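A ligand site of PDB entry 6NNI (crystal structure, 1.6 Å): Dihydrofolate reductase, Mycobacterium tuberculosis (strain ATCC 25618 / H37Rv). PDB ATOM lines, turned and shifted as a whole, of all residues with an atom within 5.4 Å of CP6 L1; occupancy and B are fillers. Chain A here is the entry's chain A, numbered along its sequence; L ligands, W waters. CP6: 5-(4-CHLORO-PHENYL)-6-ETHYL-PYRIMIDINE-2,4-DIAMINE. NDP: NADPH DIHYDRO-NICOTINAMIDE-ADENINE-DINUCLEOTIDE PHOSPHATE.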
ATOM      1  N   ILE A   5      17.990  17.032  -0.854  1.00  0.00           N
ATOM      2  CA  ILE A   5      18.575  15.734  -1.204  1.00  0.00           C
ATOM      3  C   ILE A   5      19.705  15.973  -2.207  1.00  0.00           C
ATOM      4  O   ILE A   5      19.524  16.690  -3.203  1.00  0.00           O
ATOM      5  CB  ILE A   5      17.506  14.748  -1.737  1.00  0.00           C
ATOM      6  CG1 ILE A   5      18.136  13.378  -2.029  1.00  0.00           C
ATOM      7  CG2 ILE A   5      16.732  15.323  -2.935  1.00  0.00           C
ATOM      8  CD1 ILE A   5      17.085  12.244  -2.152  1.00  0.00           C
ATOM      9  N   TRP A   6      20.874  15.413  -1.903  1.00  0.00           N
ATOM     10  CA  TRP A   6      22.046  15.615  -2.766  1.00  0.00           C
ATOM     11  C   TRP A   6      23.011  14.464  -2.588  1.00  0.00           C
ATOM     12  O   TRP A   6      22.972  13.739  -1.595  1.00  0.00           O
ATOM     13  CB  TRP A   6      22.754  16.952  -2.469  1.00  0.00           C
ATOM     14  CG  TRP A   6      23.550  17.028  -1.194  1.00  0.00           C
ATOM     15  CD1 TRP A   6      24.817  16.544  -0.980  1.00  0.00           C
ATOM     16  CD2 TRP A   6      23.164  17.660   0.038  1.00  0.00           C
ATOM     17  NE1 TRP A   6      25.230  16.824   0.306  1.00  0.00           N
ATOM     18  CE2 TRP A   6      24.232  17.519   0.937  1.00  0.00           C
ATOM     19  CE3 TRP A   6      22.014  18.350   0.449  1.00  0.00           C
ATOM     20  CZ2 TRP A   6      24.181  18.014   2.234  1.00  0.00           C
ATOM     21  CZ3 TRP A   6      21.969  18.852   1.741  1.00  0.00           C
ATOM     22  CH2 TRP A   6      23.052  18.681   2.618  1.00  0.00           C
ATOM     23  N   ALA A   7      23.889  14.307  -3.577  1.00  0.00           N
ATOM     24  CA  ALA A   7      25.010  13.401  -3.480  1.00  0.00           C
ATOM     25  C   ALA A   7      26.281  14.241  -3.532  1.00  0.00           C
ATOM     26  O   ALA A   7      26.374  15.162  -4.346  1.00  0.00           O
ATOM     27  CB  ALA A   7      24.992  12.376  -4.627  1.00  0.00           C
ATOM     28  N   ILE A  20      27.924  16.378 -13.116  1.00  0.00           N
ATOM     29  CA  ILE A  20      28.355  15.646 -11.933  1.00  0.00           C
ATOM     30  C   ILE A  20      29.461  14.661 -12.300  1.00  0.00           C
ATOM     31  O   ILE A  20      29.304  13.950 -13.295  1.00  0.00           O
ATOM     32  CB  ILE A  20      27.162  14.918 -11.304  1.00  0.00           C
ATOM     33  CG1 ILE A  20      26.023  15.916 -11.018  1.00  0.00           C
ATOM     34  CG2 ILE A  20      27.564  14.195 -10.003  1.00  0.00           C
ATOM     35  CD1 ILE A  20      24.733  15.221 -10.677  1.00  0.00           C
ATOM     36  N   ASP A  27      22.360   5.409  -6.186  1.00  0.00           N
ATOM     37  CA  ASP A  27      21.995   6.755  -5.739  1.00  0.00           C
ATOM     38  C   ASP A  27      20.843   7.290  -6.561  1.00  0.00           C
ATOM     39  O   ASP A  27      19.932   7.940  -6.028  1.00  0.00           O
ATOM     40  CB  ASP A  27      23.212   7.667  -5.839  1.00  0.00           C
ATOM     41  CG  ASP A  27      22.871   9.106  -5.506  1.00  0.00           C
ATOM     42  OD1 ASP A  27      22.418   9.349  -4.379  1.00  0.00           O
ATOM     43  OD2 ASP A  27      23.075   9.971  -6.387  1.00  0.00           O
ATOM     44  N   GLN A  28      20.838   7.001  -7.869  1.00  0.00           N
ATOM     45  CA  GLN A  28      19.720   7.418  -8.687  1.00  0.00           C
ATOM     46  C   GLN A  28      18.429   6.770  -8.205  1.00  0.00           C
ATOM     47  O   GLN A  28      17.397   7.431  -8.098  1.00  0.00           O
ATOM     48  CB  GLN A  28      19.984   7.064 -10.156  1.00  0.00           C
ATOM     49  CG  GLN A  28      19.137   7.934 -11.071  1.00  0.00           C
ATOM     50  CD  GLN A  28      18.612   7.195 -12.282  1.00  0.00           C
ATOM     51  OE1 GLN A  28      19.353   6.904 -13.222  1.00  0.00           O
ATOM     52  NE2 GLN A  28      17.327   6.870 -12.253  1.00  0.00           N
ATOM     53  N   HIS A  30      17.772   5.666  -5.180  1.00  0.00           N
ATOM     54  CA  HIS A  30      17.459   6.273  -3.897  1.00  0.00           C
ATOM     55  C   HIS A  30      16.807   7.643  -4.093  1.00  0.00           C
ATOM     56  O   HIS A  30      15.758   7.938  -3.501  1.00  0.00           O
ATOM     57  CB  HIS A  30      18.747   6.370  -3.076  1.00  0.00           C
ATOM     58  CG  HIS A  30      18.639   7.209  -1.855  1.00  0.00           C
ATOM     59  ND1 HIS A  30      17.893   6.834  -0.751  1.00  0.00           N
ATOM     60  CD2 HIS A  30      19.215   8.391  -1.532  1.00  0.00           C
ATOM     61  CE1 HIS A  30      18.005   7.767   0.180  1.00  0.00           C
ATOM     62  NE2 HIS A  30      18.806   8.718  -0.264  1.00  0.00           N
ATOM     63  N   PHE A  31      17.396   8.460  -4.977  1.00  0.00           N
ATOM     64  CA  PHE A  31      16.827   9.771  -5.255  1.00  0.00           C
ATOM     65  C   PHE A  31      15.416   9.647  -5.791  1.00  0.00           C
ATOM     66  O   PHE A  31      14.515  10.384  -5.373  1.00  0.00           O
ATOM     67  CB  PHE A  31      17.713  10.519  -6.272  1.00  0.00           C
ATOM     68  CG  PHE A  31      17.041  11.736  -6.851  1.00  0.00           C
ATOM     69  CD1 PHE A  31      17.054  12.951  -6.165  1.00  0.00           C
ATOM     70  CD2 PHE A  31      16.356  11.652  -8.069  1.00  0.00           C
ATOM     71  CE1 PHE A  31      16.397  14.044  -6.690  1.00  0.00           C
ATOM     72  CE2 PHE A  31      15.692  12.746  -8.601  1.00  0.00           C
ATOM     73  CZ  PHE A  31      15.706  13.954  -7.903  1.00  0.00           C
ATOM     74  N   THR A  46      20.361  23.499 -12.862  1.00  0.00           N
ATOM     75  CA  THR A  46      20.138  22.069 -12.705  1.00  0.00           C
ATOM     76  C   THR A  46      19.097  21.561 -13.703  1.00  0.00           C
ATOM     77  O   THR A  46      19.248  20.465 -14.266  1.00  0.00           O
ATOM     78  CB  THR A  46      19.749  21.776 -11.263  1.00  0.00           C
ATOM     79  OG1 THR A  46      20.888  22.034 -10.422  1.00  0.00           O
ATOM     80  CG2 THR A  46      19.322  20.321 -11.071  1.00  0.00           C
ATOM     81  N   SER A  49      20.815  21.010 -16.919  1.00  0.00           N
ATOM     82  CA  SER A  49      21.640  19.810 -16.966  1.00  0.00           C
ATOM     83  C   SER A  49      20.853  18.564 -17.355  1.00  0.00           C
ATOM     84  O   SER A  49      21.463  17.555 -17.699  1.00  0.00           O
ATOM     85  CB  SER A  49      22.333  19.591 -15.613  1.00  0.00           C
ATOM     86  OG  SER A  49      21.466  18.992 -14.680  1.00  0.00           O
ATOM     87  N   LEU A  50      19.530  18.599 -17.258  1.00  0.00           N
ATOM     88  CA  LEU A  50      18.712  17.449 -17.657  1.00  0.00           C
ATOM     89  C   LEU A  50      18.486  17.443 -19.171  1.00  0.00           C
ATOM     90  O   LEU A  50      18.059  18.458 -19.716  1.00  0.00           O
ATOM     91  CB  LEU A  50      17.342  17.483 -16.973  1.00  0.00           C
ATOM     92  CG  LEU A  50      17.282  17.219 -15.478  1.00  0.00           C
ATOM     93  CD1 LEU A  50      15.951  17.700 -14.925  1.00  0.00           C
ATOM     94  CD2 LEU A  50      17.500  15.737 -15.165  1.00  0.00           C
ATOM     95  N   LEU A  57      11.018  15.333 -14.709  1.00  0.00           N
ATOM     96  CA  LEU A  57      11.184  14.042 -14.064  1.00  0.00           C
ATOM     97  C   LEU A  57       9.808  13.479 -13.728  1.00  0.00           C
ATOM     98  O   LEU A  57       8.959  14.192 -13.163  1.00  0.00           O
ATOM     99  CB  LEU A  57      12.038  14.190 -12.809  1.00  0.00           C
ATOM    100  CG  LEU A  57      13.455  14.689 -13.080  1.00  0.00           C
ATOM    101  CD1 LEU A  57      14.266  14.727 -11.797  1.00  0.00           C
ATOM    102  CD2 LEU A  57      14.141  13.802 -14.142  1.00  0.00           C
ATOM    103  N   VAL A  93      14.028  19.767  -2.351  1.00  0.00           N
ATOM    104  CA  VAL A  93      14.935  20.627  -3.096  1.00  0.00           C
ATOM    105  C   VAL A  93      16.073  19.763  -3.609  1.00  0.00           C
ATOM    106  O   VAL A  93      16.784  19.113  -2.822  1.00  0.00           O
ATOM    107  CB  VAL A  93      15.461  21.766  -2.202  1.00  0.00           C
ATOM    108  CG1 VAL A  93      16.553  22.538  -2.951  1.00  0.00           C
ATOM    109  CG2 VAL A  93      14.322  22.697  -1.823  1.00  0.00           C
ATOM    110  N   ILE A  94      16.224  19.697  -4.929  1.00  0.00           N
ATOM    111  CA  ILE A  94      17.088  18.692  -5.540  1.00  0.00           C
ATOM    112  C   ILE A  94      18.359  19.295  -6.124  1.00  0.00           C
ATOM    113  O   ILE A  94      19.114  18.590  -6.808  1.00  0.00           O
ATOM    114  CB  ILE A  94      16.315  17.880  -6.590  1.00  0.00           C
ATOM    115  CG1 ILE A  94      15.939  18.726  -7.799  1.00  0.00           C
ATOM    116  CG2 ILE A  94      15.083  17.256  -5.948  1.00  0.00           C
ATOM    117  CD1 ILE A  94      15.650  17.874  -9.071  1.00  0.00           C
ATOM    118  N   GLY A  95      18.625  20.574  -5.868  1.00  0.00           N
ATOM    119  CA  GLY A  95      19.885  21.230  -6.214  1.00  0.00           C
ATOM    120  C   GLY A  95      19.666  22.386  -7.160  1.00  0.00           C
ATOM    121  O   GLY A  95      18.549  22.664  -7.592  1.00  0.00           O
ATOM    122  N   TYR A 100      20.394  25.010  -2.734  1.00  0.00           N
ATOM    123  CA  TYR A 100      20.497  24.465  -1.381  1.00  0.00           C
ATOM    124  C   TYR A 100      20.729  25.559  -0.361  1.00  0.00           C
ATOM    125  O   TYR A 100      20.147  25.534   0.728  1.00  0.00           O
ATOM    126  CB  TYR A 100      21.633  23.443  -1.259  1.00  0.00           C
ATOM    127  CG  TYR A 100      21.412  22.164  -2.028  1.00  0.00           C
ATOM    128  CD1 TYR A 100      20.194  21.496  -1.991  1.00  0.00           C
ATOM    129  CD2 TYR A 100      22.427  21.628  -2.813  1.00  0.00           C
ATOM    130  CE1 TYR A 100      19.985  20.335  -2.711  1.00  0.00           C
ATOM    131  CE2 TYR A 100      22.229  20.488  -3.555  1.00  0.00           C
ATOM    132  CZ  TYR A 100      21.024  19.831  -3.487  1.00  0.00           C
ATOM    133  OH  TYR A 100      20.855  18.716  -4.241  1.00  0.00           O
ATOM    134  N   GLU A 111      18.828  14.439   2.994  1.00  0.00           N
ATOM    135  CA  GLU A 111      19.132  13.062   2.621  1.00  0.00           C
ATOM    136  C   GLU A 111      20.383  13.134   1.757  1.00  0.00           C
ATOM    137  O   GLU A 111      20.340  13.608   0.622  1.00  0.00           O
ATOM    138  CB  GLU A 111      17.956  12.415   1.888  1.00  0.00           C
ATOM    139  CG  GLU A 111      16.770  12.121   2.795  1.00  0.00           C
ATOM    140  CD  GLU A 111      17.079  11.052   3.836  1.00  0.00           C
ATOM    141  OE1 GLU A 111      17.937  10.195   3.575  1.00  0.00           O
ATOM    142  OE2 GLU A 111      16.483  11.057   4.929  1.00  0.00           O
ATOM    143  N   THR A 113      23.835  11.459   0.060  1.00  0.00           N
ATOM    144  CA  THR A 113      24.659  10.332  -0.353  1.00  0.00           C
ATOM    145  C   THR A 113      26.091  10.816  -0.366  1.00  0.00           C
ATOM    146  O   THR A 113      26.416  11.791  -1.066  1.00  0.00           O
ATOM    147  CB  THR A 113      24.269   9.830  -1.742  1.00  0.00           C
ATOM    148  OG1 THR A 113      22.887   9.469  -1.733  1.00  0.00           O
ATOM    149  CG2 THR A 113      25.131   8.635  -2.163  1.00  0.00           C
HETATM  150  N1  CP6 L   1      20.424  13.828  -5.045  1.00  0.00           N
HETATM  151  C2  CP6 L   1      21.044  12.669  -5.133  1.00  0.00           C
HETATM  152  C3  CP6 L   1      20.181  14.541  -6.137  1.00  0.00           C
HETATM  153  C4  CP6 L   1      20.583  14.079  -7.389  1.00  0.00           C
HETATM  154  C5  CP6 L   1      21.237  12.857  -7.420  1.00  0.00           C
HETATM  155  N6  CP6 L   1      21.454  12.211  -6.290  1.00  0.00           N
HETATM  156  C7  CP6 L   1      20.301  14.806  -8.568  1.00  0.00           C
HETATM  157  C8  CP6 L   1      19.013  14.730  -9.080  1.00  0.00           C
HETATM  158  C9  CP6 L   1      18.648  15.424 -10.237  1.00  0.00           C
HETATM  159  C10 CP6 L   1      19.603  16.203 -10.870  1.00  0.00           C
HETATM  160  C11 CP6 L   1      20.894  16.279 -10.376  1.00  0.00           C
HETATM  161  C12 CP6 L   1      21.242  15.574  -9.233  1.00  0.00           C
HETATM  162  N13 CP6 L   1      19.507  15.791  -5.993  1.00  0.00           N
HETATM  163  N14 CP6 L   1      21.305  11.902  -3.951  1.00  0.00           N
HETATM  164  C15 CP6 L   1      21.728  12.192  -8.695  1.00  0.00           C
HETATM  165  C16 CP6 L   1      20.922  10.908  -8.894  1.00  0.00           C
HETATM  166 CL1  CP6 L   1      19.145  17.067 -12.354  1.00  0.00          CL
HETATM  167  PA  NDP L   2      21.647  25.963  -9.396  1.00  0.00           P
HETATM  168  O1A NDP L   2      21.179  24.667  -9.967  1.00  0.00           O
HETATM  169  O2A NDP L   2      21.580  26.235  -7.928  1.00  0.00           O
HETATM  170  O5B NDP L   2      20.796  27.053 -10.287  1.00  0.00           O
HETATM  171  C5B NDP L   2      21.329  28.380 -10.144  1.00  0.00           C
HETATM  172  C4B NDP L   2      20.261  29.278 -10.793  1.00  0.00           C
HETATM  173  O4B NDP L   2      19.122  29.343  -9.924  1.00  0.00           O
HETATM  174  C3B NDP L   2      20.717  30.738 -11.045  1.00  0.00           C
HETATM  175  O3B NDP L   2      21.454  30.839 -12.239  1.00  0.00           O
HETATM  176  C2B NDP L   2      19.314  31.403 -11.219  1.00  0.00           C
HETATM  177  O2B NDP L   2      18.685  31.081 -12.343  1.00  0.00           O
HETATM  178  C1B NDP L   2      18.525  30.662 -10.083  1.00  0.00           C
HETATM  179  N9A NDP L   2      18.659  31.363  -8.846  1.00  0.00           N
HETATM  180  C8A NDP L   2      19.714  31.359  -7.942  1.00  0.00           C
HETATM  181  N7A NDP L   2      19.499  32.180  -6.889  1.00  0.00           N
HETATM  182  C5A NDP L   2      18.239  32.736  -7.142  1.00  0.00           C
HETATM  183  C6A NDP L   2      17.443  33.660  -6.439  1.00  0.00           C
HETATM  184  N6A NDP L   2      17.876  34.197  -5.236  1.00  0.00           N
HETATM  185  N1A NDP L   2      16.222  34.038  -6.921  1.00  0.00           N
HETATM  186  C2A NDP L   2      15.853  33.472  -8.109  1.00  0.00           C
HETATM  187  N3A NDP L   2      16.488  32.570  -8.887  1.00  0.00           N
HETATM  188  C4A NDP L   2      17.705  32.241  -8.365  1.00  0.00           C
HETATM  189  O3  NDP L   2      23.179  26.193 -10.049  1.00  0.00           O
HETATM  190  PN  NDP L   2      24.515  25.659  -9.319  1.00  0.00           P
HETATM  191  O1N NDP L   2      25.537  25.976 -10.342  1.00  0.00           O
HETATM  192  O2N NDP L   2      24.729  26.103  -7.885  1.00  0.00           O
HETATM  193  O5D NDP L   2      24.390  23.940  -9.207  1.00  0.00           O
HETATM  194  C5D NDP L   2      24.455  23.342 -10.462  1.00  0.00           C
HETATM  195  C4D NDP L   2      25.499  22.232 -10.360  1.00  0.00           C
HETATM  196  O4D NDP L   2      25.100  21.316  -9.326  1.00  0.00           O
HETATM  197  C3D NDP L   2      25.575  21.420 -11.660  1.00  0.00           C
HETATM  198  O3D NDP L   2      26.918  21.012 -11.762  1.00  0.00           O
HETATM  199  C2D NDP L   2      24.679  20.213 -11.359  1.00  0.00           C
HETATM  200  O2D NDP L   2      25.054  19.072 -12.106  1.00  0.00           O
HETATM  201  C1D NDP L   2      25.043  19.996  -9.879  1.00  0.00           C
HETATM  202  N1N NDP L   2      24.003  19.232  -9.141  1.00  0.00           N
HETATM  203  C2N NDP L   2      24.399  18.158  -8.367  1.00  0.00           C
HETATM  204  C3N NDP L   2      23.541  17.574  -7.485  1.00  0.00           C
HETATM  205  C7N NDP L   2      23.966  16.439  -6.679  1.00  0.00           C
HETATM  206  O7N NDP L   2      23.227  15.906  -5.855  1.00  0.00           O
HETATM  207  N7N NDP L   2      25.239  15.906  -6.844  1.00  0.00           N
HETATM  208  C4N NDP L   2      22.161  18.071  -7.330  1.00  0.00           C
HETATM  209  C5N NDP L   2      21.764  19.073  -8.361  1.00  0.00           C
HETATM  210  C6N NDP L   2      22.652  19.609  -9.210  1.00  0.00           C
HETATM  211  P2B NDP L   2      18.807  32.246 -13.689  1.00  0.00           P
HETATM  212  O1X NDP L   2      17.964  31.550 -14.707  1.00  0.00           O
HETATM  213  O2X NDP L   2      20.318  32.292 -13.985  1.00  0.00           O
HETATM  214  O3X NDP L   2      18.216  33.445 -13.014  1.00  0.00           O
HETATM  215  O   HOH W   1      20.722  11.236  -1.111  1.00  0.00           O
HETATM  216  O   HOH W   2      23.667  10.615 -10.975  1.00  0.00           O
HETATM  217  O   HOH W   3      22.927  17.659 -12.805  1.00  0.00           O
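O of Trp 6 sits close to N14 of CP6 L1, 3.4 Å away.
A nitrogen (N7N) of NDP L2 lies within hydrogen-bond range of the backbone carbonyl oxygen of Ala 7 (2.8 Å).
O of Ile 5 lies within hydrogen-bond range of N13 of CP6 L1 (2.9 Å).
An oxygen (O7N) of NDP L2 sits at hydrogen-bond distance from the backbone NH (N) of Ala 7 (2.9 Å).
OG1 of Thr 46 sits at hydrogen-bond distance from O1A of NDP L2 (2.7 Å).
N of Thr 46 sits at hydrogen-bond distance from O1A of NDP L2 (3.2 Å).
A nitrogen (N6) of CP6 L1 sits at hydrogen-bond distance from the side-chain carboxylate of Asp 27 (2.8 Å).
A nitrogen (N13) of CP6 L1 sits at hydrogen-bond distance from the backbone carbonyl oxygen (O) of Ile 94, 2.9 Å away.
O of Ile 5 lies within hydrogen-bond range of OH of Tyr 100 (2.6 Å).
The backbone carbonyl oxygen of Trp 6 sits at hydrogen-bond distance from the backbone NH of Thr 113 (2.9 Å).
N of Ile 5 is in hydrogen-bond range of O of Val 93, at 3.1 Å.
The side-chain hydroxyl (OG1) of Thr 113 sits at hydrogen-bond distance from the side-chain carboxylate (OD1) of Asp 27 (2.7 Å).
The backbone carbonyl oxygen (O) of Thr 46 sits at hydrogen-bond distance from the side-chain hydroxyl (OG) of Ser 49 (2.7 Å).
The backbone NH (N) of Trp 6 is in hydrogen-bond range of the backbone carbonyl oxygen (O) of Glu 111 (3.1 Å).
O of Ile 94 is in hydrogen-bond range of OH of Tyr 100.
The backbone NH (N) of Gly 95 lies within hydrogen-bond range of the side-chain hydroxyl (OH) of Tyr 100.
Residues that only touch CP6 L1: Ala 7, Ile 20, Gln 28, Phe 31, Thr 46, Ser 49, Leu 50, Tyr 100 and Thr 113.
Hydrophobic or aromatic side chains within 4 Å of CP6 L1: Ile 5, Ala 7, Ile 20, Phe 31, Leu 50 and Ile 94.
Within 4 Å of CP6 L1: Ile 5, Trp 6, Ala 7, Ile 20, Asp 27, Gln 28, Phe 31, Thr 46, Ser 49, Leu 50, Ile 94, Tyr 100 and Thr 113.
The nearest printed residue that does not touch CP6 L1 is Leu 57 (4.7 Å).
Water W1 lies within hydrogen-bond range of the side-chain hydroxyl (OG1) of Thr 113, the backbone carbonyl oxygen (O) of Glu 111, a nitrogen (N14) of CP6 L1, a ring nitrogen (NE2) of His 30 and the backbone carbonyl oxygen (O) of Trp 6.
Water W3 lies within hydrogen-bond range of O2D of NDP L2 (2.6 Å) and OG of Ser 49 (2.7 Å).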
